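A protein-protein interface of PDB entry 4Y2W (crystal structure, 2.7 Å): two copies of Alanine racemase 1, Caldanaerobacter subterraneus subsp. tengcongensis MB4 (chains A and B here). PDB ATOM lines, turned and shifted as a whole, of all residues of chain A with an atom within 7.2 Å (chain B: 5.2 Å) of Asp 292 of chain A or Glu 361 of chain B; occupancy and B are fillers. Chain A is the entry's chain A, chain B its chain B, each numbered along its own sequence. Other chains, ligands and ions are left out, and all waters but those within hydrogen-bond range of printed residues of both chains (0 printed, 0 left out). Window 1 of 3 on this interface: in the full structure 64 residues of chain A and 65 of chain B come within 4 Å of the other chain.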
ATOM      1  N   GLY A 286     -21.240  -7.180 -21.128  1.00  0.00           N
ATOM      2  CA  GLY A 286     -22.632  -6.883 -21.456  1.00  0.00           C
ATOM      3  C   GLY A 286     -23.501  -8.118 -21.348  1.00  0.00           C
ATOM      4  O   GLY A 286     -23.088  -9.114 -20.759  1.00  0.00           O
ATOM      5  N   TYR A 287     -24.701  -8.061 -21.923  1.00  0.00           N
ATOM      6  CA  TYR A 287     -25.672  -9.150 -21.750  1.00  0.00           C
ATOM      7  C   TYR A 287     -25.352 -10.410 -22.551  1.00  0.00           C
ATOM      8  O   TYR A 287     -25.805 -11.500 -22.195  1.00  0.00           O
ATOM      9  CB  TYR A 287     -27.115  -8.685 -22.001  1.00  0.00           C
ATOM     10  CG  TYR A 287     -27.397  -8.003 -23.325  1.00  0.00           C
ATOM     11  CD1 TYR A 287     -27.480  -8.731 -24.508  1.00  0.00           C
ATOM     12  CD2 TYR A 287     -27.631  -6.631 -23.382  1.00  0.00           C
ATOM     13  CE1 TYR A 287     -27.760  -8.107 -25.714  1.00  0.00           C
ATOM     14  CE2 TYR A 287     -27.914  -6.001 -24.581  1.00  0.00           C
ATOM     15  CZ  TYR A 287     -27.977  -6.742 -25.743  1.00  0.00           C
ATOM     16  OH  TYR A 287     -28.249  -6.109 -26.931  1.00  0.00           O
ATOM     17  N   ALA A 288     -24.564 -10.273 -23.611  1.00  0.00           N
ATOM     18  CA  ALA A 288     -24.119 -11.433 -24.372  1.00  0.00           C
ATOM     19  C   ALA A 288     -23.105 -12.261 -23.585  1.00  0.00           C
ATOM     20  O   ALA A 288     -22.842 -13.413 -23.933  1.00  0.00           O
ATOM     21  CB  ALA A 288     -23.525 -10.998 -25.699  1.00  0.00           C
ATOM     22  N   ASP A 289     -22.534 -11.666 -22.537  1.00  0.00           N
ATOM     23  CA  ASP A 289     -21.591 -12.355 -21.659  1.00  0.00           C
ATOM     24  C   ASP A 289     -22.264 -13.021 -20.464  1.00  0.00           C
ATOM     25  O   ASP A 289     -21.627 -13.803 -19.753  1.00  0.00           O
ATOM     26  CB  ASP A 289     -20.531 -11.375 -21.162  1.00  0.00           C
ATOM     27  CG  ASP A 289     -19.684 -10.820 -22.286  1.00  0.00           C
ATOM     28  OD1 ASP A 289     -19.271 -11.605 -23.161  1.00  0.00           O
ATOM     29  OD2 ASP A 289     -19.419  -9.599 -22.304  1.00  0.00           O
ATOM     30  N   GLY A 290     -23.543 -12.716 -20.247  1.00  0.00           N
ATOM     31  CA  GLY A 290     -24.296 -13.242 -19.108  1.00  0.00           C
ATOM     32  C   GLY A 290     -24.675 -12.217 -18.051  1.00  0.00           C
ATOM     33  O   GLY A 290     -25.108 -12.588 -16.961  1.00  0.00           O
ATOM     34  N   LEU A 291     -24.509 -10.932 -18.357  1.00  0.00           N
ATOM     35  CA  LEU A 291     -24.931  -9.873 -17.443  1.00  0.00           C
ATOM     36  C   LEU A 291     -26.329  -9.416 -17.833  1.00  0.00           C
ATOM     37  O   LEU A 291     -26.495  -8.701 -18.815  1.00  0.00           O
ATOM     38  CB  LEU A 291     -23.952  -8.698 -17.483  1.00  0.00           C
ATOM     39  CG  LEU A 291     -24.195  -7.634 -16.413  1.00  0.00           C
ATOM     40  CD1 LEU A 291     -24.059  -8.246 -15.026  1.00  0.00           C
ATOM     41  CD2 LEU A 291     -23.246  -6.456 -16.582  1.00  0.00           C
ATOM     42  N   ASP A 292     -27.330  -9.824 -17.060  1.00  0.00           N
ATOM     43  CA  ASP A 292     -28.725  -9.615 -17.442  1.00  0.00           C
ATOM     44  C   ASP A 292     -29.048  -8.138 -17.633  1.00  0.00           C
ATOM     45  O   ASP A 292     -28.737  -7.303 -16.789  1.00  0.00           O
ATOM     46  CB  ASP A 292     -29.675 -10.227 -16.410  1.00  0.00           C
ATOM     47  CG  ASP A 292     -31.096 -10.332 -16.919  1.00  0.00           C
ATOM     48  OD1 ASP A 292     -31.634  -9.331 -17.431  1.00  0.00           O
ATOM     49  OD2 ASP A 292     -31.679 -11.426 -16.820  1.00  0.00           O
ATOM     50  N   ARG A 293     -29.699  -7.839 -18.750  1.00  0.00           N
ATOM     51  CA  ARG A 293     -30.044  -6.473 -19.116  1.00  0.00           C
ATOM     52  C   ARG A 293     -31.001  -5.806 -18.116  1.00  0.00           C
ATOM     53  O   ARG A 293     -31.054  -4.576 -18.036  1.00  0.00           O
ATOM     54  CB  ARG A 293     -30.644  -6.461 -20.523  1.00  0.00           C
ATOM     55  CG  ARG A 293     -30.849  -5.082 -21.113  1.00  0.00           C
ATOM     56  CD  ARG A 293     -31.060  -5.160 -22.615  1.00  0.00           C
ATOM     57  NE  ARG A 293     -31.755  -3.981 -23.122  1.00  0.00           N
ATOM     58  CZ  ARG A 293     -33.070  -3.788 -23.062  1.00  0.00           C
ATOM     59  NH1 ARG A 293     -33.872  -4.699 -22.517  1.00  0.00           N
ATOM     60  NH2 ARG A 293     -33.591  -2.670 -23.549  1.00  0.00           N
ATOM     61  N   ARG A 294     -31.745  -6.607 -17.352  1.00  0.00           N
ATOM     62  CA  ARG A 294     -32.646  -6.067 -16.323  1.00  0.00           C
ATOM     63  C   ARG A 294     -31.903  -5.386 -15.164  1.00  0.00           C
ATOM     64  O   ARG A 294     -32.514  -4.642 -14.402  1.00  0.00           O
ATOM     65  CB  ARG A 294     -33.615  -7.142 -15.799  1.00  0.00           C
ATOM     66  CG  ARG A 294     -34.816  -7.358 -16.715  1.00  0.00           C
ATOM     67  CD  ARG A 294     -35.752  -8.454 -16.229  1.00  0.00           C
ATOM     68  NE  ARG A 294     -35.082  -9.753 -16.201  1.00  0.00           N
ATOM     69  CZ  ARG A 294     -35.125 -10.632 -15.195  1.00  0.00           C
ATOM     70  NH1 ARG A 294     -35.848 -10.405 -14.093  1.00  0.00           N
ATOM     71  NH2 ARG A 294     -34.453 -11.776 -15.307  1.00  0.00           N
ATOM     72  N   LEU A 295     -30.596  -5.625 -15.050  1.00  0.00           N
ATOM     73  CA  LEU A 295     -29.757  -4.917 -14.079  1.00  0.00           C
ATOM     74  C   LEU A 295     -29.467  -3.464 -14.481  1.00  0.00           C
ATOM     75  O   LEU A 295     -28.838  -2.731 -13.720  1.00  0.00           O
ATOM     76  CB  LEU A 295     -28.436  -5.659 -13.865  1.00  0.00           C
ATOM     77  CG  LEU A 295     -28.521  -7.115 -13.400  1.00  0.00           C
ATOM     78  CD1 LEU A 295     -27.121  -7.666 -13.192  1.00  0.00           C
ATOM     79  CD2 LEU A 295     -29.337  -7.255 -12.126  1.00  0.00           C
ATOM     80  N   SER A 296     -29.907  -3.059 -15.672  1.00  0.00           N
ATOM     81  CA  SER A 296     -29.881  -1.653 -16.082  1.00  0.00           C
ATOM     82  C   SER A 296     -30.415  -0.751 -14.969  1.00  0.00           C
ATOM     83  O   SER A 296     -31.580  -0.872 -14.585  1.00  0.00           O
ATOM     84  CB  SER A 296     -30.744  -1.460 -17.334  1.00  0.00           C
ATOM     85  OG  SER A 296     -30.300  -2.270 -18.411  1.00  0.00           O
ATOM     86  N   ASN A 298     -30.069  -0.801 -11.770  1.00  0.00           N
ATOM     87  CA  ASN A 298     -30.390  -1.400 -10.465  1.00  0.00           C
ATOM     88  C   ASN A 298     -29.510  -2.595 -10.137  1.00  0.00           C
ATOM     89  O   ASN A 298     -29.989  -3.707  -9.899  1.00  0.00           O
ATOM     90  CB  ASN A 298     -31.884  -1.759 -10.318  1.00  0.00           C
ATOM     91  CG  ASN A 298     -32.342  -2.795 -11.321  1.00  0.00           C
ATOM     92  OD1 ASN A 298     -31.834  -2.848 -12.437  1.00  0.00           O
ATOM     93  ND2 ASN A 298     -33.306  -3.622 -10.931  1.00  0.00           N
ATOM     94  N   ILE A 310     -24.500   0.418 -11.771  1.00  0.00           N
ATOM     95  CA  ILE A 310     -24.635   0.413 -13.217  1.00  0.00           C
ATOM     96  C   ILE A 310     -25.518   1.592 -13.592  1.00  0.00           C
ATOM     97  O   ILE A 310     -26.626   1.722 -13.081  1.00  0.00           O
ATOM     98  CB  ILE A 310     -25.275  -0.895 -13.723  1.00  0.00           C
ATOM     99  CG1 ILE A 310     -24.333  -2.075 -13.478  1.00  0.00           C
ATOM    100  CG2 ILE A 310     -25.605  -0.800 -15.208  1.00  0.00           C
ATOM    101  CD1 ILE A 310     -24.988  -3.431 -13.640  1.00  0.00           C
ATOM    102  N   VAL A 314     -27.695  -1.730 -19.894  1.00  0.00           N
ATOM    103  CA  VAL A 314     -26.632  -2.688 -20.152  1.00  0.00           C
ATOM    104  C   VAL A 314     -26.652  -3.002 -21.643  1.00  0.00           C
ATOM    105  O   VAL A 314     -27.678  -3.412 -22.186  1.00  0.00           O
ATOM    106  CB  VAL A 314     -26.810  -3.976 -19.323  1.00  0.00           C
ATOM    107  CG1 VAL A 314     -25.791  -5.032 -19.725  1.00  0.00           C
ATOM    108  CG2 VAL A 314     -26.690  -3.665 -17.841  1.00  0.00           C
ATOM    109  N   MET A 316     -24.884  -4.943 -25.161  1.00  0.00           N
ATOM    110  CA  MET A 316     -24.587  -6.333 -25.477  1.00  0.00           C
ATOM    111  C   MET A 316     -23.202  -6.751 -24.987  1.00  0.00           C
ATOM    112  O   MET A 316     -23.015  -7.877 -24.522  1.00  0.00           O
ATOM    113  CB  MET A 316     -24.683  -6.538 -26.987  1.00  0.00           C
ATOM    114  CG  MET A 316     -24.614  -7.985 -27.444  1.00  0.00           C
ATOM    115  SD  MET A 316     -25.228  -8.160 -29.130  1.00  0.00           S
ATOM    116  CE  MET A 316     -24.679  -9.823 -29.504  1.00  0.00           C
ATOM    117  N   MET A 351     -27.343 -11.766  -6.693  1.00  0.00           N
ATOM    118  CA  MET A 351     -27.673 -11.527  -8.094  1.00  0.00           C
ATOM    119  C   MET A 351     -28.940 -12.280  -8.499  1.00  0.00           C
ATOM    120  O   MET A 351     -29.814 -11.721  -9.160  1.00  0.00           O
ATOM    121  CB  MET A 351     -26.507 -11.926  -8.999  1.00  0.00           C
ATOM    122  CG  MET A 351     -26.792 -11.742 -10.484  1.00  0.00           C
ATOM    123  SD  MET A 351     -25.316 -11.464 -11.483  1.00  0.00           S
ATOM    124  CE  MET A 351     -24.962  -9.758 -11.066  1.00  0.00           C
ATOM    125  N   ILE A 355     -32.820 -10.486  -9.832  1.00  0.00           N
ATOM    126  CA  ILE A 355     -33.554 -10.791 -11.073  1.00  0.00           C
ATOM    127  C   ILE A 355     -34.555 -11.948 -10.923  1.00  0.00           C
ATOM    128  O   ILE A 355     -34.954 -12.559 -11.914  1.00  0.00           O
ATOM    129  CB  ILE A 355     -32.609 -11.035 -12.280  1.00  0.00           C
ATOM    130  CG1 ILE A 355     -31.496 -12.032 -11.937  1.00  0.00           C
ATOM    131  CG2 ILE A 355     -32.007  -9.718 -12.742  1.00  0.00           C
ATOM    132  CD1 ILE A 355     -30.860 -12.682 -13.149  1.00  0.00           C
ATOM    133  N   THR A 357     -34.646 -15.128  -9.615  1.00  0.00           N
ATOM    134  CA  THR A 357     -34.301 -16.479 -10.036  1.00  0.00           C
ATOM    135  C   THR A 357     -33.442 -17.148  -8.961  1.00  0.00           C
ATOM    136  O   THR A 357     -33.416 -16.699  -7.816  1.00  0.00           O
ATOM    137  CB  THR A 357     -33.596 -16.475 -11.413  1.00  0.00           C
ATOM    138  OG1 THR A 357     -33.430 -17.820 -11.875  1.00  0.00           O
ATOM    139  CG2 THR A 357     -32.232 -15.791 -11.339  1.00  0.00           C
ATOM    140  N   GLU A 361     -29.361 -20.636 -12.496  1.00  0.00           N
ATOM    141  CA  GLU A 361     -29.581 -19.941 -13.771  1.00  0.00           C
ATOM    142  C   GLU A 361     -28.572 -18.813 -14.016  1.00  0.00           C
ATOM    143  O   GLU A 361     -28.195 -18.556 -15.162  1.00  0.00           O
ATOM    144  CB  GLU A 361     -31.005 -19.390 -13.874  1.00  0.00           C
ATOM    145  CG  GLU A 361     -31.345 -18.859 -15.264  1.00  0.00           C
ATOM    146  CD  GLU A 361     -32.784 -18.396 -15.401  1.00  0.00           C
ATOM    147  OE1 GLU A 361     -33.321 -17.769 -14.460  1.00  0.00           O
ATOM    148  OE2 GLU A 361     -33.378 -18.645 -16.467  1.00  0.00           O
ATOM    149  N   ARG A 365     -25.900 -18.563 -17.192  1.00  0.00           N
ATOM    150  CA  ARG A 365     -26.008 -17.411 -18.075  1.00  0.00           C
ATOM    151  C   ARG A 365     -24.634 -16.945 -18.576  1.00  0.00           C
ATOM    152  O   ARG A 365     -24.546 -16.259 -19.594  1.00  0.00           O
ATOM    153  CB  ARG A 365     -26.697 -16.263 -17.331  1.00  0.00           C
ATOM    154  CG  ARG A 365     -27.890 -15.656 -18.048  1.00  0.00           C
ATOM    155  CD  ARG A 365     -29.042 -16.643 -18.174  1.00  0.00           C
ATOM    156  NE  ARG A 365     -30.336 -15.998 -17.973  1.00  0.00           N
ATOM    157  CZ  ARG A 365     -31.515 -16.604 -18.110  1.00  0.00           C
ATOM    158  NH1 ARG A 365     -31.595 -17.889 -18.474  1.00  0.00           N
ATOM    159  NH2 ARG A 365     -32.628 -15.913 -17.888  1.00  0.00           N
ATOM    160  N   ARG B 294     -38.290 -17.664 -16.170  1.00  0.00           N
ATOM    161  CA  ARG B 294     -39.528 -16.898 -16.009  1.00  0.00           C
ATOM    162  C   ARG B 294     -40.604 -17.255 -17.037  1.00  0.00           C
ATOM    163  O   ARG B 294     -41.706 -16.728 -16.965  1.00  0.00           O
ATOM    164  CB  ARG B 294     -39.247 -15.389 -16.038  1.00  0.00           C
ATOM    165  CG  ARG B 294     -38.625 -14.871 -14.751  1.00  0.00           C
ATOM    166  CD  ARG B 294     -38.080 -13.462 -14.901  1.00  0.00           C
ATOM    167  NE  ARG B 294     -37.073 -13.403 -15.958  1.00  0.00           N
ATOM    168  CZ  ARG B 294     -37.075 -12.561 -16.992  1.00  0.00           C
ATOM    169  NH1 ARG B 294     -38.020 -11.629 -17.131  1.00  0.00           N
ATOM    170  NH2 ARG B 294     -36.093 -12.627 -17.888  1.00  0.00           N
ATOM    171  N   THR B 357     -37.216  -7.986 -22.516  1.00  0.00           N
ATOM    172  CA  THR B 357     -35.897  -7.610 -23.009  1.00  0.00           C
ATOM    173  C   THR B 357     -35.995  -7.410 -24.527  1.00  0.00           C
ATOM    174  O   THR B 357     -37.095  -7.230 -25.058  1.00  0.00           O
ATOM    175  CB  THR B 357     -34.816  -8.658 -22.638  1.00  0.00           C
ATOM    176  OG1 THR B 357     -33.519  -8.168 -23.007  1.00  0.00           O
ATOM    177  CG2 THR B 357     -35.064  -9.995 -23.333  1.00  0.00           C
ATOM    178  N   ILE B 358     -34.853  -7.435 -25.214  1.00  0.00           N
ATOM    179  CA  ILE B 358     -34.808  -7.241 -26.667  1.00  0.00           C
ATOM    180  C   ILE B 358     -34.234  -8.480 -27.358  1.00  0.00           C
ATOM    181  O   ILE B 358     -33.476  -9.231 -26.743  1.00  0.00           O
ATOM    182  CB  ILE B 358     -33.998  -5.985 -27.063  1.00  0.00           C
ATOM    183  CG1 ILE B 358     -32.647  -5.934 -26.338  1.00  0.00           C
ATOM    184  CG2 ILE B 358     -34.790  -4.722 -26.764  1.00  0.00           C
ATOM    185  CD1 ILE B 358     -31.783  -4.759 -26.747  1.00  0.00           C
ATOM    186  N   PRO B 359     -34.594  -8.696 -28.642  1.00  0.00           N
ATOM    187  CA  PRO B 359     -34.174  -9.864 -29.423  1.00  0.00           C
ATOM    188  C   PRO B 359     -32.707 -10.266 -29.284  1.00  0.00           C
ATOM    189  O   PRO B 359     -32.397 -11.460 -29.271  1.00  0.00           O
ATOM    190  CB  PRO B 359     -34.446  -9.426 -30.860  1.00  0.00           C
ATOM    191  CG  PRO B 359     -35.614  -8.515 -30.753  1.00  0.00           C
ATOM    192  CD  PRO B 359     -35.498  -7.826 -29.424  1.00  0.00           C
ATOM    193  N   GLN B 360     -31.819  -9.282 -29.188  1.00  0.00           N
ATOM    194  CA  GLN B 360     -30.382  -9.550 -29.128  1.00  0.00           C
ATOM    195  C   GLN B 360     -30.025 -10.354 -27.884  1.00  0.00           C
ATOM    196  O   GLN B 360     -29.200 -11.258 -27.948  1.00  0.00           O
ATOM    197  CB  GLN B 360     -29.563  -8.255 -29.150  1.00  0.00           C
ATOM    198  CG  GLN B 360     -29.704  -7.416 -30.414  1.00  0.00           C
ATOM    199  CD  GLN B 360     -30.855  -6.428 -30.362  1.00  0.00           C
ATOM    200  OE1 GLN B 360     -31.733  -6.531 -29.516  1.00  0.00           O
ATOM    201  NE2 GLN B 360     -30.856  -5.470 -31.269  1.00  0.00           N
ATOM    202  N   GLU B 361     -30.645 -10.029 -26.752  1.00  0.00           N
ATOM    203  CA  GLU B 361     -30.385 -10.782 -25.530  1.00  0.00           C
ATOM    204  C   GLU B 361     -30.958 -12.199 -25.610  1.00  0.00           C
ATOM    205  O   GLU B 361     -30.365 -13.133 -25.080  1.00  0.00           O
ATOM    206  CB  GLU B 361     -30.909 -10.058 -24.290  1.00  0.00           C
ATOM    207  CG  GLU B 361     -30.387 -10.688 -23.006  1.00  0.00           C
ATOM    208  CD  GLU B 361     -30.738  -9.920 -21.755  1.00  0.00           C
ATOM    209  OE1 GLU B 361     -31.803  -9.263 -21.712  1.00  0.00           O
ATOM    210  OE2 GLU B 361     -29.944  -9.999 -20.796  1.00  0.00           O
ATOM    211  N   VAL B 362     -32.098 -12.355 -26.279  1.00  0.00           N
ATOM    212  CA  VAL B 362     -32.701 -13.676 -26.435  1.00  0.00           C
ATOM    213  C   VAL B 362     -31.755 -14.567 -27.230  1.00  0.00           C
ATOM    214  O   VAL B 362     -31.404 -15.650 -26.777  1.00  0.00           O
ATOM    215  CB  VAL B 362     -34.094 -13.623 -27.105  1.00  0.00           C
ATOM    216  CG1 VAL B 362     -34.647 -15.031 -27.306  1.00  0.00           C
ATOM    217  CG2 VAL B 362     -35.061 -12.806 -26.262  1.00  0.00           C
ATOM    218  N   PHE B 363     -31.326 -14.095 -28.398  1.00  0.00           N
ATOM    219  CA  PHE B 363     -30.344 -14.823 -29.216  1.00  0.00           C
ATOM    220  C   PHE B 363     -29.037 -15.110 -28.470  1.00  0.00           C
ATOM    221  O   PHE B 363     -28.453 -16.178 -28.634  1.00  0.00           O
ATOM    222  CB  PHE B 363     -30.001 -14.051 -30.497  1.00  0.00           C
ATOM    223  CG  PHE B 363     -31.054 -14.117 -31.577  1.00  0.00           C
ATOM    224  CD1 PHE B 363     -31.802 -15.267 -31.801  1.00  0.00           C
ATOM    225  CD2 PHE B 363     -31.258 -13.027 -32.412  1.00  0.00           C
ATOM    226  CE1 PHE B 363     -32.750 -15.311 -32.811  1.00  0.00           C
ATOM    227  CE2 PHE B 363     -32.206 -13.065 -33.425  1.00  0.00           C
ATOM    228  CZ  PHE B 363     -32.955 -14.210 -33.624  1.00  0.00           C
ATOM    229  N   SER B 364     -28.585 -14.155 -27.660  1.00  0.00           N
ATOM    230  CA  SER B 364     -27.320 -14.290 -26.936  1.00  0.00           C
ATOM    231  C   SER B 364     -27.386 -15.311 -25.805  1.00  0.00           C
ATOM    232  O   SER B 364     -26.361 -15.847 -25.388  1.00  0.00           O
ATOM    233  CB  SER B 364     -26.892 -12.944 -26.346  1.00  0.00           C
ATOM    234  OG  SER B 364     -27.546 -12.694 -25.106  1.00  0.00           O
ATOM    235  N   ARG B 365     -28.590 -15.560 -25.301  1.00  0.00           N
ATOM    236  CA  ARG B 365     -28.784 -16.439 -24.157  1.00  0.00           C
ATOM    237  C   ARG B 365     -28.686 -17.916 -24.559  1.00  0.00           C
ATOM    238  O   ARG B 365     -28.424 -18.785 -23.714  1.00  0.00           O
ATOM    239  CB  ARG B 365     -30.138 -16.158 -23.495  1.00  0.00           C
ATOM    240  CG  ARG B 365     -30.089 -16.246 -21.982  1.00  0.00           C
ATOM    241  CD  ARG B 365     -29.848 -14.891 -21.333  1.00  0.00           C
ATOM    242  NE  ARG B 365     -31.114 -14.233 -21.014  1.00  0.00           N
ATOM    243  CZ  ARG B 365     -31.235 -13.135 -20.271  1.00  0.00           C
ATOM    244  NH1 ARG B 365     -30.160 -12.537 -19.764  1.00  0.00           N
ATOM    245  NH2 ARG B 365     -32.439 -12.629 -20.038  1.00  0.00           N
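Tyr 287 of chain A touches Ile 358 of chain B (OH to CD1, 3.8 Å).
Tyr 287 of chain A touches Gln 360 of chain B.
Tyr 287 of chain A touches Glu 361 of chain B (CB to OE2, 3.3 Å).
O of Tyr 287 of chain A touches OG of Ser 364 of chain B, 3.6 Å away.
Ser 364 of chain B touches Ala 288 of chain A.
Glu 361 of chain B touches Asp 292 of chain A.
Thr 357 of chain B touches Arg 293 of chain A (OG1 to NH1, 3.5 Å).
Ile 358 of chain B touches Arg 293 of chain A (CD1 to NE, 3.7 Å).
Arg 365 of chain A touches Arg 365 of chain B.
Arg 294 of chain A touches its own counterpart, Arg 294 of chain B.
Arg 365 of chain A touches its own counterpart, Arg 365 of chain B.
Of the 12 pairs that touch across the chains among the printed residues, 2 have their exchanged pair printed and touching as well.
Of the 20 printed residues of chain A, 6 touch a printed residue of chain B.
Of the 10 printed residues of chain B, 7 touch a printed residue of chain A.
Among the printed residues, 12 pairs touch across the chains.
Among the printed residues, Asp or Glu carboxylates within 4 Å of a Lys or Arg side-chain nitrogen of the other chain: Asp 292 of chain A with Arg 365 of chain B (3.5 Å).
Glu 361 of chain B touches just these residues of chain A: Tyr 287, Asp 292 and Arg 293.
Printed residues of chain B within 4 Å of Arg 365 of chain A: Arg 365 (3.6 Å).
Printed residues of chain A within 4 Å of Arg 365 of chain B: Asp 292 and Arg 365.
Of the printed residues of chain A, Thr 357 of chain B touches Arg 293.
Of the printed residues of chain B, Arg 294 of chain A touches Arg 294.
Ile 310 of chain A touches none of the printed residues of chain B.
The nearest residue of chain B that does not touch Asp 292 of chain A is Arg 294 of chain B (4.7 Å).
The nearest residue of chain A that does not touch Glu 361 of chain B is Leu 291 of chain A (4.2 Å).
The side-chain carboxylate (OD2) of Asp 292 of chain A lies within salt-bridge range of the guanidinium group (NH1) of Arg 365 of chain B (3.5 Å).
The backbone NH (N) of Arg 293 of chain A sits at hydrogen-bond distance from the side-chain carboxylate (OE2) of Glu 361 of chain B (3.0 Å).
The guanidinium group (NE) of Arg 294 of chain B lies close to the guanidinium group (NH2) of Arg 294 of chain A, at 3.2 Å.
N of Tyr 287 of chain A lies within hydrogen-bond range of O of Met 316 of chain A, at 3.1 Å.
The backbone NH (N) of Ala 288 of chain A is in hydrogen-bond range of the backbone carbonyl oxygen (O) of Met 316 of chain A, 3.0 Å away.
OG of Ser 296 of chain A is in hydrogen-bond range of O of Arg 293 of chain A.
NH1 of Arg 294 of chain A lies within hydrogen-bond range of O of Ile 355 of chain A, 3.2 Å away.
OG1 of Thr 357 of chain B lies within hydrogen-bond range of OE1 of Glu 361 of chain B (2.4 Å).
The guanidinium group (NH1) of Arg 365 of chain B lies within salt-bridge range of the side-chain carboxylate (OE2) of Glu 361 of chain B, at 2.7 Å.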
